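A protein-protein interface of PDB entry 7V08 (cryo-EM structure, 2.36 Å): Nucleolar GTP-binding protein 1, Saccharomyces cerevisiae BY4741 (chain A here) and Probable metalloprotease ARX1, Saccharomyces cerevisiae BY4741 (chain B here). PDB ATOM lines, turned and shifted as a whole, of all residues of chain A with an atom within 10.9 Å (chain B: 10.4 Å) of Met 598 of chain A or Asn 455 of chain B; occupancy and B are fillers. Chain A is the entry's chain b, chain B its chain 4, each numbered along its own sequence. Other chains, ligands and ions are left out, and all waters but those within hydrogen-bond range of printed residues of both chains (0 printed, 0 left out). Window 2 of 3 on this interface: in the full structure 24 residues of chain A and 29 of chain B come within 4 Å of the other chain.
O of Ala 594 of chain A lies within hydrogen-bond range of N of Ala 462 of chain B (3.3 Å).
N of Gly 596 of chain A lies within hydrogen-bond range of O of Tyr 460 of chain B.
OD1 of Asn 455 of chain B sits close to SD of Met 598 of chain A, at 3.7 Å.
The side-chain hydroxyl (OG) of Ser 459 of chain B sits at hydrogen-bond distance from the backbone carbonyl oxygen (O) of Gly 456 of chain B (2.9 Å).
O of Val 593 of chain A is in hydrogen-bond range of NE of Arg 599 of chain A, 2.7 Å away.
The backbone carbonyl oxygen (O) of Leu 590 of chain A lies within hydrogen-bond range of the guanidinium group (NH2) of Arg 599 of chain A, 3.0 Å away.
OE1 of Glu 578 of chain A lies within salt-bridge range of NH1 of Arg 599 of chain A (3.6 Å).
O of Ser 597 of chain A is in hydrogen-bond range of OG of Ser 600 of chain A (2.6 Å).
The side-chain hydroxyl (OG) of Ser 600 of chain A lies within hydrogen-bond range of the backbone carbonyl oxygen (O) of Gly 596 of chain A.
Of chain A, only Asp 595, Ser 597 and Met 598 come within 4 Å of Asn 455 of chain B.
Gly 596 of chain A touches just these residues of chain B: Tyr 460 and Ala 462.
Of chain B, only Asn 455, Leu 458, Ser 459 and Tyr 460 come within 4 Å of Ser 597 of chain A.
Lys 601 of chain A touches none of the printed residues of chain B.
No residue of chain B comes within 4 Å of Ala 602 of chain A.
Asn 453 of chain B touches none of the printed residues of chain A.
No residue of chain A comes within 4 Å of Pro 454 of chain B.
No residue of chain A comes within 4 Å of Gly 456 of chain B.
Leu 458 of chain B touches just one residue of chain A: Ser 597 (3.3 Å).
Ser 459 of chain B touches just these residues of chain A: Asp 595 and Ser 597.
Printed residues of chain A within 4 Å of Ile 483 of chain B: Asp 595.
Printed residues of chain A within 4 Å of Tyr 460 of chain B: Asp 595, Gly 596 and Ser 597.
Printed residues of chain A within 4 Å of Asp 461 of chain B: Ala 594.
The nearest residue of chain A that does not touch Asn 455 of chain B is Lys 601 of chain A (5.1 Å).
Along chain B the printed residues that touch a printed residue of chain A span positions 455 to 483.
Of the 20 printed residues of chain A, 6 touch a printed residue of chain B.
Printed residues of chain A that touch a printed residue of chain B: Ala 594, Asp 595, Gly 596, Ser 597, Met 598 and Arg 599.
Hydrophobic or aromatic side chains of chain A that line the printed part of chain B: Met 598.
Among the printed residues, 14 pairs touch across the chains.
Among the printed residues, pairs that only touch across the chains: Ala 594 of chain A with Asp 461 of chain B, Asp 595 of chain A with Asn 455 of chain B, Asp 595 of chain A with Ser 459 of chain B, Asp 595 of chain A with Tyr 460 of chain B, Asp 595 of chain A with Ile 483 of chain B, Gly 596 of chain A with Ala 462 of chain B, Ser 597 of chain A with Asn 455 of chain B, Ser 597 of chain A with Leu 458 of chain B, Ser 597 of chain A with Ser 459 of chain B, Ser 597 of chain A with Tyr 460 of chain B and Arg 599 of chain A with Ala 462 of chain B.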
ATOM      1  N   GLU A 578      15.226  27.905   9.574  1.00  0.00           N
ATOM      2  CA  GLU A 578      14.546  28.735   8.585  1.00  0.00           C
ATOM      3  C   GLU A 578      14.832  30.219   8.791  1.00  0.00           C
ATOM      4  O   GLU A 578      14.705  31.005   7.848  1.00  0.00           O
ATOM      5  CB  GLU A 578      13.041  28.470   8.623  1.00  0.00           C
ATOM      6  CG  GLU A 578      12.644  27.021   8.367  1.00  0.00           C
ATOM      7  CD  GLU A 578      12.646  26.160   9.625  1.00  0.00           C
ATOM      8  OE1 GLU A 578      13.712  26.020  10.261  1.00  0.00           O
ATOM      9  OE2 GLU A 578      11.573  25.626   9.980  1.00  0.00           O
ATOM     10  N   LEU A 589       8.171  33.295  15.169  1.00  0.00           N
ATOM     11  CA  LEU A 589       7.276  33.041  14.052  1.00  0.00           C
ATOM     12  C   LEU A 589       6.896  31.568  13.953  1.00  0.00           C
ATOM     13  O   LEU A 589       5.756  31.249  13.617  1.00  0.00           O
ATOM     14  CB  LEU A 589       7.940  33.519  12.761  1.00  0.00           C
ATOM     15  CG  LEU A 589       7.170  33.556  11.446  1.00  0.00           C
ATOM     16  CD1 LEU A 589       6.175  34.698  11.426  1.00  0.00           C
ATOM     17  CD2 LEU A 589       8.138  33.667  10.286  1.00  0.00           C
ATOM     18  N   LEU A 590       7.825  30.664  14.274  1.00  0.00           N
ATOM     19  CA  LEU A 590       7.665  29.249  13.966  1.00  0.00           C
ATOM     20  C   LEU A 590       7.620  28.321  15.173  1.00  0.00           C
ATOM     21  O   LEU A 590       7.443  27.114  14.985  1.00  0.00           O
ATOM     22  CB  LEU A 590       8.800  28.783  13.046  1.00  0.00           C
ATOM     23  CG  LEU A 590       8.965  29.554  11.741  1.00  0.00           C
ATOM     24  CD1 LEU A 590      10.143  29.031  10.945  1.00  0.00           C
ATOM     25  CD2 LEU A 590       7.684  29.481  10.936  1.00  0.00           C
ATOM     26  N   ASP A 591       7.762  28.829  16.400  1.00  0.00           N
ATOM     27  CA  ASP A 591       7.889  27.928  17.544  1.00  0.00           C
ATOM     28  C   ASP A 591       6.592  27.189  17.847  1.00  0.00           C
ATOM     29  O   ASP A 591       6.620  26.150  18.511  1.00  0.00           O
ATOM     30  CB  ASP A 591       8.350  28.691  18.784  1.00  0.00           C
ATOM     31  CG  ASP A 591       9.855  28.699  18.935  1.00  0.00           C
ATOM     32  OD1 ASP A 591      10.544  28.025  18.139  1.00  0.00           O
ATOM     33  OD2 ASP A 591      10.352  29.380  19.853  1.00  0.00           O
ATOM     34  N   GLY A 592       5.459  27.713  17.399  1.00  0.00           N
ATOM     35  CA  GLY A 592       4.191  27.051  17.597  1.00  0.00           C
ATOM     36  C   GLY A 592       3.792  26.026  16.557  1.00  0.00           C
ATOM     37  O   GLY A 592       2.768  25.367  16.736  1.00  0.00           O
ATOM     38  N   VAL A 593       4.545  25.875  15.468  1.00  0.00           N
ATOM     39  CA  VAL A 593       4.229  24.912  14.414  1.00  0.00           C
ATOM     40  C   VAL A 593       5.351  23.884  14.386  1.00  0.00           C
ATOM     41  O   VAL A 593       6.426  24.141  13.831  1.00  0.00           O
ATOM     42  CB  VAL A 593       4.060  25.579  13.040  1.00  0.00           C
ATOM     43  CG1 VAL A 593       3.408  24.617  12.069  1.00  0.00           C
ATOM     44  CG2 VAL A 593       3.245  26.855  13.153  1.00  0.00           C
ATOM     45  N   ALA A 594       5.088  22.703  14.944  1.00  0.00           N
ATOM     46  CA  ALA A 594       6.145  21.719  15.153  1.00  0.00           C
ATOM     47  C   ALA A 594       6.584  21.040  13.859  1.00  0.00           C
ATOM     48  O   ALA A 594       7.780  20.798  13.668  1.00  0.00           O
ATOM     49  CB  ALA A 594       5.694  20.675  16.172  1.00  0.00           C
ATOM     50  N   ASP A 595       5.662  20.722  12.955  1.00  0.00           N
ATOM     51  CA  ASP A 595       6.029  19.927  11.791  1.00  0.00           C
ATOM     52  C   ASP A 595       6.137  20.769  10.522  1.00  0.00           C
ATOM     53  O   ASP A 595       5.427  21.766  10.345  1.00  0.00           O
ATOM     54  CB  ASP A 595       5.057  18.766  11.577  1.00  0.00           C
ATOM     55  CG  ASP A 595       3.673  19.217  11.254  1.00  0.00           C
ATOM     56  OD1 ASP A 595       3.246  20.253  11.797  1.00  0.00           O
ATOM     57  OD2 ASP A 595       3.007  18.525  10.460  1.00  0.00           O
ATOM     58  N   GLY A 596       7.045  20.340   9.637  1.00  0.00           N
ATOM     59  CA  GLY A 596       7.410  21.140   8.481  1.00  0.00           C
ATOM     60  C   GLY A 596       6.340  21.215   7.413  1.00  0.00           C
ATOM     61  O   GLY A 596       6.275  22.199   6.672  1.00  0.00           O
ATOM     62  N   SER A 597       5.482  20.201   7.324  1.00  0.00           N
ATOM     63  CA  SER A 597       4.364  20.260   6.389  1.00  0.00           C
ATOM     64  C   SER A 597       3.401  21.386   6.759  1.00  0.00           C
ATOM     65  O   SER A 597       2.983  22.176   5.902  1.00  0.00           O
ATOM     66  CB  SER A 597       3.647  18.910   6.356  1.00  0.00           C
ATOM     67  OG  SER A 597       2.628  18.881   5.375  1.00  0.00           O
ATOM     68  N   MET A 598       3.059  21.493   8.046  1.00  0.00           N
ATOM     69  CA  MET A 598       2.190  22.580   8.480  1.00  0.00           C
ATOM     70  C   MET A 598       2.908  23.921   8.428  1.00  0.00           C
ATOM     71  O   MET A 598       2.268  24.947   8.163  1.00  0.00           O
ATOM     72  CB  MET A 598       1.647  22.310   9.880  1.00  0.00           C
ATOM     73  CG  MET A 598       0.776  21.067   9.971  1.00  0.00           C
ATOM     74  SD  MET A 598      -0.719  21.160   8.975  1.00  0.00           S
ATOM     75  CE  MET A 598      -1.794  22.093  10.064  1.00  0.00           C
ATOM     76  N   ARG A 599       4.228  23.931   8.651  1.00  0.00           N
ATOM     77  CA  ARG A 599       4.988  25.162   8.458  1.00  0.00           C
ATOM     78  C   ARG A 599       4.881  25.656   7.019  1.00  0.00           C
ATOM     79  O   ARG A 599       4.621  26.842   6.781  1.00  0.00           O
ATOM     80  CB  ARG A 599       6.456  24.953   8.843  1.00  0.00           C
ATOM     81  CG  ARG A 599       6.701  24.870  10.334  1.00  0.00           C
ATOM     82  CD  ARG A 599       8.170  24.889  10.688  1.00  0.00           C
ATOM     83  NE  ARG A 599       8.360  25.038  12.126  1.00  0.00           N
ATOM     84  CZ  ARG A 599       9.537  25.142  12.725  1.00  0.00           C
ATOM     85  NH1 ARG A 599      10.664  25.135  12.040  1.00  0.00           N
ATOM     86  NH2 ARG A 599       9.582  25.262  14.048  1.00  0.00           N
ATOM     87  N   SER A 600       5.047  24.753   6.050  1.00  0.00           N
ATOM     88  CA  SER A 600       4.955  25.138   4.645  1.00  0.00           C
ATOM     89  C   SER A 600       3.544  25.585   4.287  1.00  0.00           C
ATOM     90  O   SER A 600       3.368  26.531   3.512  1.00  0.00           O
ATOM     91  CB  SER A 600       5.402  23.981   3.751  1.00  0.00           C
ATOM     92  OG  SER A 600       4.594  22.837   3.961  1.00  0.00           O
ATOM     93  N   LYS A 601       2.528  24.930   4.856  1.00  0.00           N
ATOM     94  CA  LYS A 601       1.149  25.340   4.593  1.00  0.00           C
ATOM     95  C   LYS A 601       0.868  26.748   5.113  1.00  0.00           C
ATOM     96  O   LYS A 601       0.274  27.571   4.405  1.00  0.00           O
ATOM     97  CB  LYS A 601       0.172  24.341   5.208  1.00  0.00           C
ATOM     98  CG  LYS A 601      -1.266  24.794   5.116  1.00  0.00           C
ATOM     99  CD  LYS A 601      -2.236  23.649   5.322  1.00  0.00           C
ATOM    100  CE  LYS A 601      -2.541  23.427   6.783  1.00  0.00           C
ATOM    101  NZ  LYS A 601      -3.307  22.168   7.009  1.00  0.00           N
ATOM    102  N   ALA A 602       1.293  27.048   6.344  1.00  0.00           N
ATOM    103  CA  ALA A 602       1.076  28.384   6.893  1.00  0.00           C
ATOM    104  C   ALA A 602       1.858  29.439   6.116  1.00  0.00           C
ATOM    105  O   ALA A 602       1.381  30.566   5.931  1.00  0.00           O
ATOM    106  CB  ALA A 602       1.449  28.417   8.373  1.00  0.00           C
ATOM    107  N   ASP A 603       3.069  29.095   5.665  1.00  0.00           N
ATOM    108  CA  ASP A 603       3.848  30.022   4.847  1.00  0.00           C
ATOM    109  C   ASP A 603       3.159  30.319   3.520  1.00  0.00           C
ATOM    110  O   ASP A 603       3.127  31.473   3.074  1.00  0.00           O
ATOM    111  CB  ASP A 603       5.248  29.464   4.605  1.00  0.00           C
ATOM    112  CG  ASP A 603       6.066  30.341   3.689  1.00  0.00           C
ATOM    113  OD1 ASP A 603       6.349  31.495   4.065  1.00  0.00           O
ATOM    114  OD2 ASP A 603       6.430  29.881   2.587  1.00  0.00           O
ATOM    115  N   ARG A 604       2.600  29.290   2.874  1.00  0.00           N
ATOM    116  CA  ARG A 604       1.854  29.512   1.638  1.00  0.00           C
ATOM    117  C   ARG A 604       0.604  30.348   1.888  1.00  0.00           C
ATOM    118  O   ARG A 604       0.238  31.188   1.058  1.00  0.00           O
ATOM    119  CB  ARG A 604       1.494  28.177   0.983  1.00  0.00           C
ATOM    120  CG  ARG A 604       2.693  27.417   0.443  1.00  0.00           C
ATOM    121  CD  ARG A 604       2.293  26.297  -0.510  1.00  0.00           C
ATOM    122  NE  ARG A 604       1.695  25.157   0.175  1.00  0.00           N
ATOM    123  CZ  ARG A 604       2.391  24.184   0.747  1.00  0.00           C
ATOM    124  NH1 ARG A 604       3.715  24.191   0.746  1.00  0.00           N
ATOM    125  NH2 ARG A 604       1.746  23.186   1.341  1.00  0.00           N
ATOM    126  N   MET A 605      -0.061  30.139   3.028  1.00  0.00           N
ATOM    127  CA  MET A 605      -1.226  30.954   3.375  1.00  0.00           C
ATOM    128  C   MET A 605      -0.846  32.424   3.515  1.00  0.00           C
ATOM    129  O   MET A 605      -1.533  33.311   2.992  1.00  0.00           O
ATOM    130  CB  MET A 605      -1.867  30.447   4.669  1.00  0.00           C
ATOM    131  CG  MET A 605      -2.609  29.129   4.546  1.00  0.00           C
ATOM    132  SD  MET A 605      -3.011  28.371   6.134  1.00  0.00           S
ATOM    133  CE  MET A 605      -4.222  29.511   6.766  1.00  0.00           C
ATOM    134  N   ALA A 606       0.260  32.697   4.209  1.00  0.00           N
ATOM    135  CA  ALA A 606       0.711  34.077   4.381  1.00  0.00           C
ATOM    136  C   ALA A 606       1.093  34.713   3.043  1.00  0.00           C
ATOM    137  O   ALA A 606       0.766  35.883   2.782  1.00  0.00           O
ATOM    138  CB  ALA A 606       1.877  34.118   5.363  1.00  0.00           C
ATOM    139  N   LYS A 607       1.761  33.947   2.173  1.00  0.00           N
ATOM    140  CA  LYS A 607       2.104  34.456   0.848  1.00  0.00           C
ATOM    141  C   LYS A 607       0.860  34.774   0.025  1.00  0.00           C
ATOM    142  O   LYS A 607       0.818  35.792  -0.672  1.00  0.00           O
ATOM    143  CB  LYS A 607       2.992  33.459   0.108  1.00  0.00           C
ATOM    144  CG  LYS A 607       4.442  33.500   0.531  1.00  0.00           C
ATOM    145  CD  LYS A 607       5.292  32.621  -0.364  1.00  0.00           C
ATOM    146  CE  LYS A 607       6.779  32.886  -0.166  1.00  0.00           C
ATOM    147  NZ  LYS A 607       7.271  32.388   1.133  1.00  0.00           N
ATOM    148  N   ALA B 451      -5.473   5.270  14.305  1.00  0.00           N
ATOM    149  CA  ALA B 451      -5.092   6.671  14.336  1.00  0.00           C
ATOM    150  C   ALA B 451      -5.133   7.282  12.938  1.00  0.00           C
ATOM    151  O   ALA B 451      -4.848   6.629  11.931  1.00  0.00           O
ATOM    152  CB  ALA B 451      -3.697   6.828  14.930  1.00  0.00           C
ATOM    153  N   THR B 452      -5.478   8.567  12.890  1.00  0.00           N
ATOM    154  CA  THR B 452      -5.599   9.309  11.644  1.00  0.00           C
ATOM    155  C   THR B 452      -4.561  10.420  11.596  1.00  0.00           C
ATOM    156  O   THR B 452      -4.460  11.228  12.525  1.00  0.00           O
ATOM    157  CB  THR B 452      -7.003   9.906  11.489  1.00  0.00           C
ATOM    158  OG1 THR B 452      -7.341  10.654  12.665  1.00  0.00           O
ATOM    159  CG2 THR B 452      -8.021   8.809  11.296  1.00  0.00           C
ATOM    160  N   ASN B 453      -3.797  10.460  10.510  1.00  0.00           N
ATOM    161  CA  ASN B 453      -2.796  11.503  10.288  1.00  0.00           C
ATOM    162  C   ASN B 453      -3.160  12.297   9.043  1.00  0.00           C
ATOM    163  O   ASN B 453      -3.039  11.771   7.917  1.00  0.00           O
ATOM    164  CB  ASN B 453      -1.392  10.913  10.170  1.00  0.00           C
ATOM    165  CG  ASN B 453      -1.334   9.708   9.266  1.00  0.00           C
ATOM    166  OD1 ASN B 453      -2.323   9.000   9.091  1.00  0.00           O
ATOM    167  ND2 ASN B 453      -0.170   9.467   8.682  1.00  0.00           N
ATOM    168  N   PRO B 454      -3.612  13.545   9.186  1.00  0.00           N
ATOM    169  CA  PRO B 454      -4.060  14.309   8.009  1.00  0.00           C
ATOM    170  C   PRO B 454      -2.955  14.656   7.018  1.00  0.00           C
ATOM    171  O   PRO B 454      -3.269  15.048   5.889  1.00  0.00           O
ATOM    172  CB  PRO B 454      -4.664  15.580   8.625  1.00  0.00           C
ATOM    173  CG  PRO B 454      -4.977  15.217  10.037  1.00  0.00           C
ATOM    174  CD  PRO B 454      -3.919  14.242  10.447  1.00  0.00           C
ATOM    175  N   ASN B 455      -1.685  14.542   7.399  1.00  0.00           N
ATOM    176  CA  ASN B 455      -0.570  14.963   6.557  1.00  0.00           C
ATOM    177  C   ASN B 455       0.110  13.817   5.824  1.00  0.00           C
ATOM    178  O   ASN B 455       0.686  14.033   4.754  1.00  0.00           O
ATOM    179  CB  ASN B 455       0.472  15.704   7.399  1.00  0.00           C
ATOM    180  CG  ASN B 455      -0.083  16.956   8.039  1.00  0.00           C
ATOM    181  OD1 ASN B 455      -0.598  17.839   7.355  1.00  0.00           O
ATOM    182  ND2 ASN B 455       0.001  17.033   9.361  1.00  0.00           N
ATOM    183  N   GLY B 456       0.079  12.608   6.381  1.00  0.00           N
ATOM    184  CA  GLY B 456       0.714  11.465   5.757  1.00  0.00           C
ATOM    185  C   GLY B 456       2.219  11.587   5.634  1.00  0.00           C
ATOM    186  O   GLY B 456       2.909  11.911   6.607  1.00  0.00           O
ATOM    187  N   ASN B 457       2.730  11.346   4.422  1.00  0.00           N
ATOM    188  CA  ASN B 457       4.168  11.362   4.169  1.00  0.00           C
ATOM    189  C   ASN B 457       4.795  12.723   4.435  1.00  0.00           C
ATOM    190  O   ASN B 457       5.974  12.795   4.799  1.00  0.00           O
ATOM    191  CB  ASN B 457       4.447  10.962   2.720  1.00  0.00           C
ATOM    192  CG  ASN B 457       4.337   9.482   2.496  1.00  0.00           C
ATOM    193  OD1 ASN B 457       4.549   8.689   3.412  1.00  0.00           O
ATOM    194  ND2 ASN B 457       4.014   9.091   1.268  1.00  0.00           N
ATOM    195  N   LEU B 458       4.035  13.805   4.265  1.00  0.00           N
ATOM    196  CA  LEU B 458       4.614  15.144   4.248  1.00  0.00           C
ATOM    197  C   LEU B 458       5.057  15.631   5.623  1.00  0.00           C
ATOM    198  O   LEU B 458       5.860  16.565   5.699  1.00  0.00           O
ATOM    199  CB  LEU B 458       3.606  16.125   3.647  1.00  0.00           C
ATOM    200  CG  LEU B 458       3.104  15.734   2.256  1.00  0.00           C
ATOM    201  CD1 LEU B 458       1.798  16.434   1.938  1.00  0.00           C
ATOM    202  CD2 LEU B 458       4.152  16.053   1.204  1.00  0.00           C
ATOM    203  N   SER B 459       4.562  15.035   6.702  1.00  0.00           N
ATOM    204  CA  SER B 459       4.856  15.539   8.038  1.00  0.00           C
ATOM    205  C   SER B 459       6.251  15.119   8.488  1.00  0.00           C
ATOM    206  O   SER B 459       6.658  13.970   8.309  1.00  0.00           O
ATOM    207  CB  SER B 459       3.804  15.050   9.031  1.00  0.00           C
ATOM    208  OG  SER B 459       3.536  13.674   8.855  1.00  0.00           O
ATOM    209  N   TYR B 460       6.986  16.067   9.067  1.00  0.00           N
ATOM    210  CA  TYR B 460       8.323  15.804   9.581  1.00  0.00           C
ATOM    211  C   TYR B 460       8.656  16.841  10.641  1.00  0.00           C
ATOM    212  O   TYR B 460       8.218  17.992  10.568  1.00  0.00           O
ATOM    213  CB  TYR B 460       9.374  15.819   8.465  1.00  0.00           C
ATOM    214  CG  TYR B 460       9.539  17.154   7.776  1.00  0.00           C
ATOM    215  CD1 TYR B 460       8.707  17.521   6.728  1.00  0.00           C
ATOM    216  CD2 TYR B 460      10.534  18.038   8.161  1.00  0.00           C
ATOM    217  CE1 TYR B 460       8.854  18.732   6.094  1.00  0.00           C
ATOM    218  CE2 TYR B 460      10.689  19.251   7.533  1.00  0.00           C
ATOM    219  CZ  TYR B 460       9.847  19.593   6.498  1.00  0.00           C
ATOM    220  OH  TYR B 460       9.995  20.804   5.863  1.00  0.00           O
ATOM    221  N   ASP B 461       9.468  16.431  11.612  1.00  0.00           N
ATOM    222  CA  ASP B 461       9.818  17.301  12.730  1.00  0.00           C
ATOM    223  C   ASP B 461      10.847  18.324  12.259  1.00  0.00           C
ATOM    224  O   ASP B 461      12.006  17.981  12.007  1.00  0.00           O
ATOM    225  CB  ASP B 461      10.348  16.474  13.897  1.00  0.00           C
ATOM    226  CG  ASP B 461      10.336  17.237  15.207  1.00  0.00           C
ATOM    227  OD1 ASP B 461      10.037  18.448  15.193  1.00  0.00           O
ATOM    228  OD2 ASP B 461      10.620  16.622  16.256  1.00  0.00           O
ATOM    229  N   ALA B 462      10.426  19.582  12.142  1.00  0.00           N
ATOM    230  CA  ALA B 462      11.320  20.634  11.682  1.00  0.00           C
ATOM    231  C   ALA B 462      12.131  21.257  12.809  1.00  0.00           C
ATOM    232  O   ALA B 462      13.073  22.005  12.530  1.00  0.00           O
ATOM    233  CB  ALA B 462      10.527  21.718  10.947  1.00  0.00           C
ATOM    234  N   LEU B 473      11.143   8.072   7.883  1.00  0.00           N
ATOM    235  CA  LEU B 473       9.855   7.440   7.604  1.00  0.00           C
ATOM    236  C   LEU B 473       9.908   6.009   8.126  1.00  0.00           C
ATOM    237  O   LEU B 473      10.313   5.088   7.402  1.00  0.00           O
ATOM    238  CB  LEU B 473       9.529   7.476   6.114  1.00  0.00           C
ATOM    239  CG  LEU B 473       8.241   6.787   5.664  1.00  0.00           C
ATOM    240  CD1 LEU B 473       7.026   7.462   6.284  1.00  0.00           C
ATOM    241  CD2 LEU B 473       8.135   6.791   4.158  1.00  0.00           C
ATOM    242  N   LEU B 478       2.526   2.798   5.238  1.00  0.00           N
ATOM    243  CA  LEU B 478       1.382   3.437   5.868  1.00  0.00           C
ATOM    244  C   LEU B 478       1.448   4.957   5.853  1.00  0.00           C
ATOM    245  O   LEU B 478       0.476   5.604   6.254  1.00  0.00           O
ATOM    246  CB  LEU B 478       1.239   2.952   7.309  1.00  0.00           C
ATOM    247  CG  LEU B 478       0.738   1.519   7.448  1.00  0.00           C
ATOM    248  CD1 LEU B 478       0.814   1.082   8.897  1.00  0.00           C
ATOM    249  CD2 LEU B 478      -0.678   1.412   6.920  1.00  0.00           C
ATOM    250  N   GLY B 479       2.556   5.538   5.407  1.00  0.00           N
ATOM    251  CA  GLY B 479       2.696   6.986   5.432  1.00  0.00           C
ATOM    252  C   GLY B 479       2.710   7.581   6.824  1.00  0.00           C
ATOM    253  O   GLY B 479       2.173   8.675   7.032  1.00  0.00           O
ATOM    254  N   VAL B 480       3.315   6.885   7.783  1.00  0.00           N
ATOM    255  CA  VAL B 480       3.431   7.363   9.157  1.00  0.00           C
ATOM    256  C   VAL B 480       4.873   7.793   9.382  1.00  0.00           C
ATOM    257  O   VAL B 480       5.799   6.988   9.231  1.00  0.00           O
ATOM    258  CB  VAL B 480       3.010   6.295  10.178  1.00  0.00           C
ATOM    259  CG1 VAL B 480       3.297   6.774  11.588  1.00  0.00           C
ATOM    260  CG2 VAL B 480       1.536   5.957  10.028  1.00  0.00           C
ATOM    261  N   SER B 481       5.058   9.050   9.771  1.00  0.00           N
ATOM    262  CA  SER B 481       6.383   9.611   9.968  1.00  0.00           C
ATOM    263  C   SER B 481       6.868   9.382  11.398  1.00  0.00           C
ATOM    264  O   SER B 481       6.174   8.815  12.243  1.00  0.00           O
ATOM    265  CB  SER B 481       6.377  11.099   9.639  1.00  0.00           C
ATOM    266  OG  SER B 481       5.644  11.822  10.609  1.00  0.00           O
ATOM    267  N   ILE B 483       7.562  11.781  13.692  1.00  0.00           N
ATOM    268  CA  ILE B 483       6.876  12.643  14.653  1.00  0.00           C
ATOM    269  C   ILE B 483       5.461  12.139  14.911  1.00  0.00           C
ATOM    270  O   ILE B 483       4.974  12.159  16.050  1.00  0.00           O
ATOM    271  CB  ILE B 483       6.898  14.109  14.172  1.00  0.00           C
ATOM    272  CG1 ILE B 483       6.109  15.011  15.130  1.00  0.00           C
ATOM    273  CG2 ILE B 483       6.402  14.234  12.739  1.00  0.00           C
ATOM    274  CD1 ILE B 483       6.016  16.449  14.681  1.00  0.00           C
ATOM    275  N   LYS B 484       4.794  11.641  13.866  1.00  0.00           N
ATOM    276  CA  LYS B 484       3.490  11.016  14.048  1.00  0.00           C
ATOM    277  C   LYS B 484       3.591   9.773  14.924  1.00  0.00           C
ATOM    278  O   LYS B 484       2.759   9.571  15.817  1.00  0.00           O
ATOM    279  CB  LYS B 484       2.880  10.671  12.692  1.00  0.00           C
ATOM    280  CG  LYS B 484       1.461  10.141  12.787  1.00  0.00           C
ATOM    281  CD  LYS B 484       0.557  11.173  13.429  1.00  0.00           C
ATOM    282  CE  LYS B 484      -0.797  10.600  13.753  1.00  0.00           C
ATOM    283  NZ  LYS B 484      -1.687  11.619  14.366  1.00  0.00           N
ATOM    284  N   SER B 487       4.044  10.746  18.492  1.00  0.00           N
ATOM    285  CA  SER B 487       2.761  11.186  19.027  1.00  0.00           C
ATOM    286  C   SER B 487       1.866  10.004  19.388  1.00  0.00           C
ATOM    287  O   SER B 487       1.228  10.005  20.447  1.00  0.00           O
ATOM    288  CB  SER B 487       2.065  12.099  18.020  1.00  0.00           C
ATOM    289  OG  SER B 487       0.712  12.311  18.373  1.00  0.00           O
